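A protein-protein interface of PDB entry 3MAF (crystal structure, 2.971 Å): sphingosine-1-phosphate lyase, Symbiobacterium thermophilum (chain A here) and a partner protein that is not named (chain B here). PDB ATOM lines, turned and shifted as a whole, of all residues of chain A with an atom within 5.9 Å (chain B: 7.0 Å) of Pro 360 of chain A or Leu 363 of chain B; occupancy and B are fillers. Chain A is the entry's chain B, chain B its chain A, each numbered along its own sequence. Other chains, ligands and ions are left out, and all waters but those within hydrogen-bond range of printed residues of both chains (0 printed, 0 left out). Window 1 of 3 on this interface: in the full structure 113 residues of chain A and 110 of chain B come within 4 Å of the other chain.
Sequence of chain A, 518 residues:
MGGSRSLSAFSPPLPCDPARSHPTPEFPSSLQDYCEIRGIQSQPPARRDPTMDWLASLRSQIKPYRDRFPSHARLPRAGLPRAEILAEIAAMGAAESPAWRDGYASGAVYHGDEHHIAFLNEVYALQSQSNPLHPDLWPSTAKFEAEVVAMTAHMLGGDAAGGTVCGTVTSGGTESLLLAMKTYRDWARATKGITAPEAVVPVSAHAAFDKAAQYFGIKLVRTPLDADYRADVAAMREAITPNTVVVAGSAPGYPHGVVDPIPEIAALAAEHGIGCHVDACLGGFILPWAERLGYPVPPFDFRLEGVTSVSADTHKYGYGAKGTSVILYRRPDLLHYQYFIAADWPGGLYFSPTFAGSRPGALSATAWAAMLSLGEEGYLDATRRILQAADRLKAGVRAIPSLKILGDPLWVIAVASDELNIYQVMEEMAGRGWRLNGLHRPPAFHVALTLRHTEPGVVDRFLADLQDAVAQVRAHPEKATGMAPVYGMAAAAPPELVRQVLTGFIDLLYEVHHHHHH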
ATOM      1  N   TYR A 124     -33.949  37.369 -13.264  1.00  0.00           N
ATOM      2  CA  TYR A 124     -32.981  36.629 -12.463  1.00  0.00           C
ATOM      3  C   TYR A 124     -31.823  37.512 -12.061  1.00  0.00           C
ATOM      4  O   TYR A 124     -31.538  37.682 -10.874  1.00  0.00           O
ATOM      5  CB  TYR A 124     -32.418  35.428 -13.224  1.00  0.00           C
ATOM      6  CG  TYR A 124     -31.362  34.699 -12.425  1.00  0.00           C
ATOM      7  CD1 TYR A 124     -31.707  33.662 -11.572  1.00  0.00           C
ATOM      8  CD2 TYR A 124     -30.034  35.074 -12.489  1.00  0.00           C
ATOM      9  CE1 TYR A 124     -30.760  33.007 -10.824  1.00  0.00           C
ATOM     10  CE2 TYR A 124     -29.078  34.425 -11.746  1.00  0.00           C
ATOM     11  CZ  TYR A 124     -29.448  33.389 -10.913  1.00  0.00           C
ATOM     12  OH  TYR A 124     -28.509  32.729 -10.154  1.00  0.00           O
ATOM     13  N   SER A 130     -30.486  37.152  -4.132  1.00  0.00           N
ATOM     14  CA  SER A 130     -31.608  36.831  -3.251  1.00  0.00           C
ATOM     15  C   SER A 130     -31.525  35.460  -2.562  1.00  0.00           C
ATOM     16  O   SER A 130     -30.925  34.526  -3.086  1.00  0.00           O
ATOM     17  CB  SER A 130     -32.926  36.958  -4.014  1.00  0.00           C
ATOM     18  OG  SER A 130     -34.012  36.547  -3.205  1.00  0.00           O
ATOM     19  N   ASN A 131     -32.149  35.365  -1.389  1.00  0.00           N
ATOM     20  CA  ASN A 131     -32.153  34.157  -0.568  1.00  0.00           C
ATOM     21  C   ASN A 131     -33.224  34.260   0.520  1.00  0.00           C
ATOM     22  O   ASN A 131     -32.962  34.785   1.601  1.00  0.00           O
ATOM     23  CB  ASN A 131     -30.779  33.950   0.069  1.00  0.00           C
ATOM     24  CG  ASN A 131     -30.682  32.662   0.877  1.00  0.00           C
ATOM     25  OD1 ASN A 131     -31.684  32.004   1.147  1.00  0.00           O
ATOM     26  ND2 ASN A 131     -29.461  32.302   1.272  1.00  0.00           N
ATOM     27  N   PRO A 132     -34.437  33.753   0.228  1.00  0.00           N
ATOM     28  CA  PRO A 132     -35.661  33.844   1.043  1.00  0.00           C
ATOM     29  C   PRO A 132     -35.521  33.339   2.472  1.00  0.00           C
ATOM     30  O   PRO A 132     -36.431  33.535   3.273  1.00  0.00           O
ATOM     31  CB  PRO A 132     -36.653  32.963   0.283  1.00  0.00           C
ATOM     32  CG  PRO A 132     -36.179  32.990  -1.127  1.00  0.00           C
ATOM     33  CD  PRO A 132     -34.683  33.086  -1.063  1.00  0.00           C
ATOM     34  N   SER A 358     -31.714  27.530   2.872  1.00  0.00           N
ATOM     35  CA  SER A 358     -31.433  28.638   1.982  1.00  0.00           C
ATOM     36  C   SER A 358     -31.775  28.164   0.569  1.00  0.00           C
ATOM     37  O   SER A 358     -31.789  26.964   0.295  1.00  0.00           O
ATOM     38  CB  SER A 358     -29.988  29.144   2.137  1.00  0.00           C
ATOM     39  OG  SER A 358     -29.081  28.454   1.305  1.00  0.00           O
ATOM     40  N   ARG A 359     -32.102  29.098  -0.313  1.00  0.00           N
ATOM     41  CA  ARG A 359     -32.615  28.735  -1.623  1.00  0.00           C
ATOM     42  C   ARG A 359     -32.594  29.955  -2.547  1.00  0.00           C
ATOM     43  O   ARG A 359     -32.313  31.063  -2.101  1.00  0.00           O
ATOM     44  CB  ARG A 359     -34.023  28.148  -1.484  1.00  0.00           C
ATOM     45  CG  ARG A 359     -35.029  29.096  -0.880  1.00  0.00           C
ATOM     46  CD  ARG A 359     -36.212  28.361  -0.275  1.00  0.00           C
ATOM     47  NE  ARG A 359     -37.173  29.287   0.328  1.00  0.00           N
ATOM     48  CZ  ARG A 359     -37.170  29.659   1.609  1.00  0.00           C
ATOM     49  NH1 ARG A 359     -36.261  29.191   2.462  1.00  0.00           N
ATOM     50  NH2 ARG A 359     -38.087  30.510   2.042  1.00  0.00           N
ATOM     51  N   PRO A 360     -32.875  29.756  -3.843  1.00  0.00           N
ATOM     52  CA  PRO A 360     -32.683  30.845  -4.810  1.00  0.00           C
ATOM     53  C   PRO A 360     -33.906  31.732  -5.014  1.00  0.00           C
ATOM     54  O   PRO A 360     -34.748  31.427  -5.863  1.00  0.00           O
ATOM     55  CB  PRO A 360     -32.391  30.100  -6.117  1.00  0.00           C
ATOM     56  CG  PRO A 360     -32.311  28.630  -5.757  1.00  0.00           C
ATOM     57  CD  PRO A 360     -33.094  28.466  -4.514  1.00  0.00           C
ATOM     58  N   GLY A 361     -33.999  32.826  -4.265  1.00  0.00           N
ATOM     59  CA  GLY A 361     -35.123  33.734  -4.413  1.00  0.00           C
ATOM     60  C   GLY A 361     -35.283  34.154  -5.862  1.00  0.00           C
ATOM     61  O   GLY A 361     -36.400  34.303  -6.363  1.00  0.00           O
ATOM     62  N   ALA A 362     -34.148  34.341  -6.530  1.00  0.00           N
ATOM     63  CA  ALA A 362     -34.125  34.726  -7.929  1.00  0.00           C
ATOM     64  C   ALA A 362     -35.109  33.904  -8.746  1.00  0.00           C
ATOM     65  O   ALA A 362     -35.804  34.431  -9.606  1.00  0.00           O
ATOM     66  CB  ALA A 362     -32.726  34.589  -8.492  1.00  0.00           C
ATOM     67  N   LEU A 363     -35.179  32.607  -8.486  1.00  0.00           N
ATOM     68  CA  LEU A 363     -36.085  31.761  -9.258  1.00  0.00           C
ATOM     69  C   LEU A 363     -37.551  32.141  -9.026  1.00  0.00           C
ATOM     70  O   LEU A 363     -38.339  32.219  -9.964  1.00  0.00           O
ATOM     71  CB  LEU A 363     -35.845  30.285  -8.956  1.00  0.00           C
ATOM     72  CG  LEU A 363     -34.454  29.823  -9.380  1.00  0.00           C
ATOM     73  CD1 LEU A 363     -34.374  28.308  -9.384  1.00  0.00           C
ATOM     74  CD2 LEU A 363     -34.116  30.371 -10.744  1.00  0.00           C
ATOM     75  N   SER A 364     -37.900  32.385  -7.768  1.00  0.00           N
ATOM     76  CA  SER A 364     -39.235  32.842  -7.420  1.00  0.00           C
ATOM     77  C   SER A 364     -39.578  34.114  -8.186  1.00  0.00           C
ATOM     78  O   SER A 364     -40.669  34.245  -8.741  1.00  0.00           O
ATOM     79  CB  SER A 364     -39.332  33.094  -5.918  1.00  0.00           C
ATOM     80  OG  SER A 364     -39.260  31.876  -5.200  1.00  0.00           O
ATOM     81  N   ALA A 365     -38.645  35.055  -8.212  1.00  0.00           N
ATOM     82  CA  ALA A 365     -38.830  36.242  -9.024  1.00  0.00           C
ATOM     83  C   ALA A 365     -39.241  35.878 -10.459  1.00  0.00           C
ATOM     84  O   ALA A 365     -40.196  36.434 -10.989  1.00  0.00           O
ATOM     85  CB  ALA A 365     -37.567  37.099  -9.023  1.00  0.00           C
ATOM     86  N   VAL B 123     -23.372  33.442 -16.952  1.00  0.00           N
ATOM     87  CA  VAL B 123     -23.325  31.995 -16.991  1.00  0.00           C
ATOM     88  C   VAL B 123     -24.745  31.468 -16.950  1.00  0.00           C
ATOM     89  O   VAL B 123     -25.190  30.793 -17.877  1.00  0.00           O
ATOM     90  CB  VAL B 123     -22.569  31.425 -15.803  1.00  0.00           C
ATOM     91  CG1 VAL B 123     -22.634  29.894 -15.827  1.00  0.00           C
ATOM     92  CG2 VAL B 123     -21.126  31.935 -15.797  1.00  0.00           C
ATOM     93  N   TYR B 124     -25.460  31.795 -15.873  1.00  0.00           N
ATOM     94  CA  TYR B 124     -26.865  31.411 -15.733  1.00  0.00           C
ATOM     95  C   TYR B 124     -27.627  31.601 -17.034  1.00  0.00           C
ATOM     96  O   TYR B 124     -28.208  30.667 -17.567  1.00  0.00           O
ATOM     97  CB  TYR B 124     -27.561  32.218 -14.642  1.00  0.00           C
ATOM     98  CG  TYR B 124     -29.024  31.866 -14.547  1.00  0.00           C
ATOM     99  CD1 TYR B 124     -29.456  30.854 -13.711  1.00  0.00           C
ATOM    100  CD2 TYR B 124     -29.969  32.513 -15.323  1.00  0.00           C
ATOM    101  CE1 TYR B 124     -30.788  30.508 -13.631  1.00  0.00           C
ATOM    102  CE2 TYR B 124     -31.305  32.176 -15.249  1.00  0.00           C
ATOM    103  CZ  TYR B 124     -31.710  31.172 -14.402  1.00  0.00           C
ATOM    104  OH  TYR B 124     -33.046  30.827 -14.322  1.00  0.00           O
ATOM    105  N   GLN B 127     -26.941  28.944 -19.630  1.00  0.00           N
ATOM    106  CA  GLN B 127     -27.497  27.645 -19.298  1.00  0.00           C
ATOM    107  C   GLN B 127     -28.933  27.778 -18.825  1.00  0.00           C
ATOM    108  O   GLN B 127     -29.426  26.926 -18.086  1.00  0.00           O
ATOM    109  CB  GLN B 127     -26.654  26.970 -18.214  1.00  0.00           C
ATOM    110  CG  GLN B 127     -25.449  26.218 -18.750  1.00  0.00           C
ATOM    111  CD  GLN B 127     -25.830  24.930 -19.459  1.00  0.00           C
ATOM    112  OE1 GLN B 127     -25.548  23.837 -18.968  1.00  0.00           O
ATOM    113  NE2 GLN B 127     -26.482  25.051 -20.615  1.00  0.00           N
ATOM    114  N   SER B 128     -29.595  28.847 -19.249  1.00  0.00           N
ATOM    115  CA  SER B 128     -30.909  29.217 -18.720  1.00  0.00           C
ATOM    116  C   SER B 128     -31.887  28.035 -18.678  1.00  0.00           C
ATOM    117  O   SER B 128     -32.287  27.561 -17.604  1.00  0.00           O
ATOM    118  CB  SER B 128     -31.492  30.343 -19.566  1.00  0.00           C
ATOM    119  OG  SER B 128     -31.353  30.036 -20.949  1.00  0.00           O
ATOM    120  N   SER B 130     -32.626  24.824 -18.762  1.00  0.00           N
ATOM    121  CA  SER B 130     -31.690  23.702 -18.784  1.00  0.00           C
ATOM    122  C   SER B 130     -31.619  22.923 -17.467  1.00  0.00           C
ATOM    123  O   SER B 130     -31.000  23.390 -16.505  1.00  0.00           O
ATOM    124  CB  SER B 130     -30.287  24.184 -19.137  1.00  0.00           C
ATOM    125  OG  SER B 130     -29.325  23.290 -18.608  1.00  0.00           O
ATOM    126  N   VAL B 169     -24.351  16.650  -6.689  1.00  0.00           N
ATOM    127  CA  VAL B 169     -24.692  18.052  -6.487  1.00  0.00           C
ATOM    128  C   VAL B 169     -26.132  18.148  -5.971  1.00  0.00           C
ATOM    129  O   VAL B 169     -27.071  17.682  -6.619  1.00  0.00           O
ATOM    130  CB  VAL B 169     -24.533  18.869  -7.795  1.00  0.00           C
ATOM    131  CG1 VAL B 169     -24.973  20.298  -7.595  1.00  0.00           C
ATOM    132  CG2 VAL B 169     -23.096  18.831  -8.275  1.00  0.00           C
ATOM    133  N   SER B 171     -29.081  20.813  -3.691  1.00  0.00           N
ATOM    134  CA  SER B 171     -29.607  22.163  -3.831  1.00  0.00           C
ATOM    135  C   SER B 171     -29.287  23.035  -2.628  1.00  0.00           C
ATOM    136  O   SER B 171     -29.753  24.167  -2.545  1.00  0.00           O
ATOM    137  CB  SER B 171     -31.115  22.113  -3.994  1.00  0.00           C
ATOM    138  OG  SER B 171     -31.725  21.901  -2.733  1.00  0.00           O
ATOM    139  N   THR B 314     -21.184  24.860  -2.081  1.00  0.00           N
ATOM    140  CA  THR B 314     -20.542  25.627  -3.136  1.00  0.00           C
ATOM    141  C   THR B 314     -21.139  27.020  -3.289  1.00  0.00           C
ATOM    142  O   THR B 314     -20.545  27.882  -3.929  1.00  0.00           O
ATOM    143  CB  THR B 314     -20.647  24.914  -4.486  1.00  0.00           C
ATOM    144  OG1 THR B 314     -21.996  24.475  -4.678  1.00  0.00           O
ATOM    145  CG2 THR B 314     -19.716  23.714  -4.533  1.00  0.00           C
ATOM    146  N   GLY B 320     -20.239  30.104  -5.578  1.00  0.00           N
ATOM    147  CA  GLY B 320     -21.181  29.826  -6.638  1.00  0.00           C
ATOM    148  C   GLY B 320     -22.482  30.549  -6.338  1.00  0.00           C
ATOM    149  O   GLY B 320     -22.699  31.020  -5.220  1.00  0.00           O
ATOM    150  N   ALA B 321     -23.343  30.651  -7.345  1.00  0.00           N
ATOM    151  CA  ALA B 321     -24.650  31.267  -7.177  1.00  0.00           C
ATOM    152  C   ALA B 321     -25.487  30.431  -6.231  1.00  0.00           C
ATOM    153  O   ALA B 321     -25.296  29.223  -6.113  1.00  0.00           O
ATOM    154  CB  ALA B 321     -25.356  31.417  -8.523  1.00  0.00           C
ATOM    155  N   LYS B 322     -26.419  31.094  -5.562  1.00  0.00           N
ATOM    156  CA  LYS B 322     -27.268  30.465  -4.557  1.00  0.00           C
ATOM    157  C   LYS B 322     -28.053  29.267  -5.121  1.00  0.00           C
ATOM    158  O   LYS B 322     -28.483  29.276  -6.277  1.00  0.00           O
ATOM    159  CB  LYS B 322     -28.206  31.527  -3.958  1.00  0.00           C
ATOM    160  CG  LYS B 322     -28.739  31.219  -2.586  1.00  0.00           C
ATOM    161  CD  LYS B 322     -27.620  30.986  -1.598  1.00  0.00           C
ATOM    162  CE  LYS B 322     -26.755  32.206  -1.441  1.00  0.00           C
ATOM    163  NZ  LYS B 322     -25.739  31.977  -0.382  1.00  0.00           N
ATOM    164  N   GLY B 323     -28.212  28.231  -4.301  1.00  0.00           N
ATOM    165  CA  GLY B 323     -29.036  27.089  -4.656  1.00  0.00           C
ATOM    166  C   GLY B 323     -28.256  25.877  -5.125  1.00  0.00           C
ATOM    167  O   GLY B 323     -28.669  25.148  -6.028  1.00  0.00           O
ATOM    168  N   THR B 324     -27.123  25.629  -4.492  1.00  0.00           N
ATOM    169  CA  THR B 324     -26.222  24.635  -5.026  1.00  0.00           C
ATOM    170  C   THR B 324     -25.283  24.148  -3.922  1.00  0.00           C
ATOM    171  O   THR B 324     -24.869  24.919  -3.061  1.00  0.00           O
ATOM    172  CB  THR B 324     -25.471  25.234  -6.233  1.00  0.00           C
ATOM    173  OG1 THR B 324     -25.228  24.226  -7.213  1.00  0.00           O
ATOM    174  CG2 THR B 324     -24.175  25.887  -5.801  1.00  0.00           C
ATOM    175  N   ARG B 359     -34.341  19.736 -11.812  1.00  0.00           N
ATOM    176  CA  ARG B 359     -33.523  20.694 -11.059  1.00  0.00           C
ATOM    177  C   ARG B 359     -32.790  21.687 -11.983  1.00  0.00           C
ATOM    178  O   ARG B 359     -32.340  21.311 -13.060  1.00  0.00           O
ATOM    179  CB  ARG B 359     -32.529  19.957 -10.153  1.00  0.00           C
ATOM    180  CG  ARG B 359     -31.615  18.987 -10.874  1.00  0.00           C
ATOM    181  CD  ARG B 359     -30.313  18.778 -10.100  1.00  0.00           C
ATOM    182  NE  ARG B 359     -29.584  20.028  -9.879  1.00  0.00           N
ATOM    183  CZ  ARG B 359     -29.492  20.649  -8.704  1.00  0.00           C
ATOM    184  NH1 ARG B 359     -30.085  20.133  -7.631  1.00  0.00           N
ATOM    185  NH2 ARG B 359     -28.807  21.785  -8.602  1.00  0.00           N
ATOM    186  N   PRO B 360     -32.659  22.958 -11.560  1.00  0.00           N
ATOM    187  CA  PRO B 360     -32.099  24.023 -12.409  1.00  0.00           C
ATOM    188  C   PRO B 360     -30.621  23.801 -12.736  1.00  0.00           C
ATOM    189  O   PRO B 360     -29.743  24.181 -11.957  1.00  0.00           O
ATOM    190  CB  PRO B 360     -32.241  25.283 -11.543  1.00  0.00           C
ATOM    191  CG  PRO B 360     -33.031  24.879 -10.338  1.00  0.00           C
ATOM    192  CD  PRO B 360     -32.844  23.410 -10.175  1.00  0.00           C
ATOM    193  N   GLY B 361     -30.350  23.200 -13.888  1.00  0.00           N
ATOM    194  CA  GLY B 361     -28.985  22.955 -14.311  1.00  0.00           C
ATOM    195  C   GLY B 361     -28.192  24.240 -14.325  1.00  0.00           C
ATOM    196  O   GLY B 361     -27.018  24.258 -13.967  1.00  0.00           O
ATOM    197  N   ALA B 362     -28.844  25.320 -14.740  1.00  0.00           N
ATOM    198  CA  ALA B 362     -28.225  26.640 -14.745  1.00  0.00           C
ATOM    199  C   ALA B 362     -27.450  26.914 -13.461  1.00  0.00           C
ATOM    200  O   ALA B 362     -26.353  27.472 -13.508  1.00  0.00           O
ATOM    201  CB  ALA B 362     -29.275  27.717 -14.960  1.00  0.00           C
ATOM    202  N   LEU B 363     -28.012  26.533 -12.316  1.00  0.00           N
ATOM    203  CA  LEU B 363     -27.344  26.800 -11.049  1.00  0.00           C
ATOM    204  C   LEU B 363     -26.052  26.017 -10.937  1.00  0.00           C
ATOM    205  O   LEU B 363     -25.042  26.547 -10.501  1.00  0.00           O
ATOM    206  CB  LEU B 363     -28.267  26.512  -9.871  1.00  0.00           C
ATOM    207  CG  LEU B 363     -29.488  27.435  -9.820  1.00  0.00           C
ATOM    208  CD1 LEU B 363     -30.185  27.355  -8.478  1.00  0.00           C
ATOM    209  CD2 LEU B 363     -29.069  28.862 -10.090  1.00  0.00           C
ATOM    210  N   SER B 364     -26.083  24.758 -11.349  1.00  0.00           N
ATOM    211  CA  SER B 364     -24.876  23.939 -11.374  1.00  0.00           C
ATOM    212  C   SER B 364     -23.785  24.620 -12.200  1.00  0.00           C
ATOM    213  O   SER B 364     -22.617  24.696 -11.799  1.00  0.00           O
ATOM    214  CB  SER B 364     -25.181  22.553 -11.943  1.00  0.00           C
ATOM    215  OG  SER B 364     -26.020  21.818 -11.071  1.00  0.00           O
ATOM    216  N   ALA B 365     -24.173  25.116 -13.365  1.00  0.00           N
ATOM    217  CA  ALA B 365     -23.245  25.854 -14.195  1.00  0.00           C
ATOM    218  C   ALA B 365     -22.558  26.947 -13.371  1.00  0.00           C
ATOM    219  O   ALA B 365     -21.342  27.084 -13.415  1.00  0.00           O
ATOM    220  CB  ALA B 365     -23.962  26.440 -15.414  1.00  0.00           C
ATOM    221  N   THR B 366     -23.325  27.708 -12.601  1.00  0.00           N
ATOM    222  CA  THR B 366     -22.736  28.832 -11.881  1.00  0.00           C
ATOM    223  C   THR B 366     -21.691  28.371 -10.867  1.00  0.00           C
ATOM    224  O   THR B 366     -20.735  29.096 -10.582  1.00  0.00           O
ATOM    225  CB  THR B 366     -23.785  29.728 -11.177  1.00  0.00           C
ATOM    226  OG1 THR B 366     -24.386  29.009 -10.104  1.00  0.00           O
ATOM    227  CG2 THR B 366     -24.863  30.183 -12.147  1.00  0.00           C
ATOM    228  N   ALA B 367     -21.869  27.166 -10.330  1.00  0.00           N
ATOM    229  CA  ALA B 367     -20.899  26.604  -9.392  1.00  0.00           C
ATOM    230  C   ALA B 367     -19.620  26.171 -10.117  1.00  0.00           C
ATOM    231  O   ALA B 367     -18.503  26.440  -9.676  1.00  0.00           O
ATOM    232  CB  ALA B 367     -21.507  25.430  -8.653  1.00  0.00           C
ATOM    233  N   TRP B 368     -19.798  25.485 -11.233  1.00  0.00           N
ATOM    234  CA  TRP B 368     -18.687  25.020 -12.037  1.00  0.00           C
ATOM    235  C   TRP B 368     -17.869  26.227 -12.473  1.00  0.00           C
ATOM    236  O   TRP B 368     -16.641  26.258 -12.333  1.00  0.00           O
ATOM    237  CB  TRP B 368     -19.257  24.273 -13.242  1.00  0.00           C
ATOM    238  CG  TRP B 368     -18.272  23.716 -14.213  1.00  0.00           C
ATOM    239  CD1 TRP B 368     -17.566  22.556 -14.094  1.00  0.00           C
ATOM    240  CD2 TRP B 368     -17.923  24.271 -15.483  1.00  0.00           C
ATOM    241  NE1 TRP B 368     -16.781  22.365 -15.207  1.00  0.00           N
ATOM    242  CE2 TRP B 368     -16.983  23.405 -16.074  1.00  0.00           C
ATOM    243  CE3 TRP B 368     -18.306  25.424 -16.173  1.00  0.00           C
ATOM    244  CZ2 TRP B 368     -16.423  23.652 -17.323  1.00  0.00           C
ATOM    245  CZ3 TRP B 368     -17.749  25.670 -17.412  1.00  0.00           C
ATOM    246  CH2 TRP B 368     -16.817  24.790 -17.975  1.00  0.00           C
ATOM    247  N   ALA B 369     -18.569  27.235 -12.980  1.00  0.00           N
ATOM    248  CA  ALA B 369     -17.936  28.459 -13.451  1.00  0.00           C
ATOM    249  C   ALA B 369     -17.208  29.171 -12.325  1.00  0.00           C
ATOM    250  O   ALA B 369     -16.094  29.647 -12.496  1.00  0.00           O
ATOM    251  CB  ALA B 369     -18.974  29.378 -14.070  1.00  0.00           C
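Among the printed residues, merely in contact across the chains: Arg 359 of chain A with Lys 322 of chain B (3.6 Å), Asn 131 of chain A with Lys 322 of chain B (3.7 Å), Pro 360 of chain A with Leu 363 of chain B (3.7 Å), Tyr 124 of chain A with Tyr 124 of chain B (3.8 Å), Leu 363 of chain A with Tyr 124 of chain B (3.8 Å), Pro 360 of chain A with Gly 323 of chain B (3.8 Å), Tyr 124 of chain A with Ala 321 of chain B (3.8 Å), Leu 363 of chain A with Pro 360 of chain B (3.8 Å), Tyr 124 of chain A with Leu 363 of chain B (3.9 Å), Pro 360 of chain A with Lys 322 of chain B (3.9 Å) and Ser 130 of chain A with Lys 322 of chain B (3.996 Å).
Pro 360 of chain A touches just these residues of chain B: Lys 322, Gly 323 and Leu 363. Of chain A, only Tyr 124 (3.9 Å) and Pro 360 (3.7 Å) come within 4 Å of Leu 363 of chain B. Printed residues of chain A within 4 Å of Tyr 124 of chain B: Tyr 124 and Leu 363. Of the printed residues of chain B, Ser 130 of chain A touches Lys 322 (3.996 Å). Of the printed residues of chain B, Arg 359 of chain A touches Lys 322 (3.6 Å). Of the printed residues of chain B, Tyr 124 of chain A touches Tyr 124, Ala 321 and Leu 363. Ala 365 of chain A touches none of the printed residues of chain B. The nearest residue of chain A that does not touch Leu 363 of chain B is Leu 363 of chain A (4.4 Å). The nearest printed residue of chain A that does not touch Ala 321 of chain B is Pro 360 of chain A (6.9 Å).
N of Ala 321 of chain B lies close to OG1 of Thr 366 of chain B (3.4 Å). The backbone carbonyl oxygen (O) of Leu 363 of chain B lies within hydrogen-bond range of the side-chain hydroxyl (OG1) of Thr 366 of chain B, at 2.6 Å. The side-chain amide oxygen (OD1) of Asn 131 of chain A sits at hydrogen-bond distance from the backbone NH (N) of Arg 359 of chain A, at 3.3 Å.
Hydrophobic or aromatic side chains of chain A that line the printed part of chain B: Tyr 124, Pro 360 and Leu 363. Of the 24 printed residues of chain B, 6 touch a printed residue of chain A. Printed residues of chain B that touch a printed residue of chain A: Tyr 124, Ala 321, Lys 322, Gly 323, Pro 360 and Leu 363. Hydrophobic or aromatic side chains of chain B that line the printed part of chain A: Tyr 124, Ala 321, Pro 360 and Leu 363. Among the printed residues, 11 pairs touch across the chains. Among the printed residues, no Asp or Glu carboxylate lies within 4 Å of a Lys or Arg side-chain nitrogen of the other chain.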
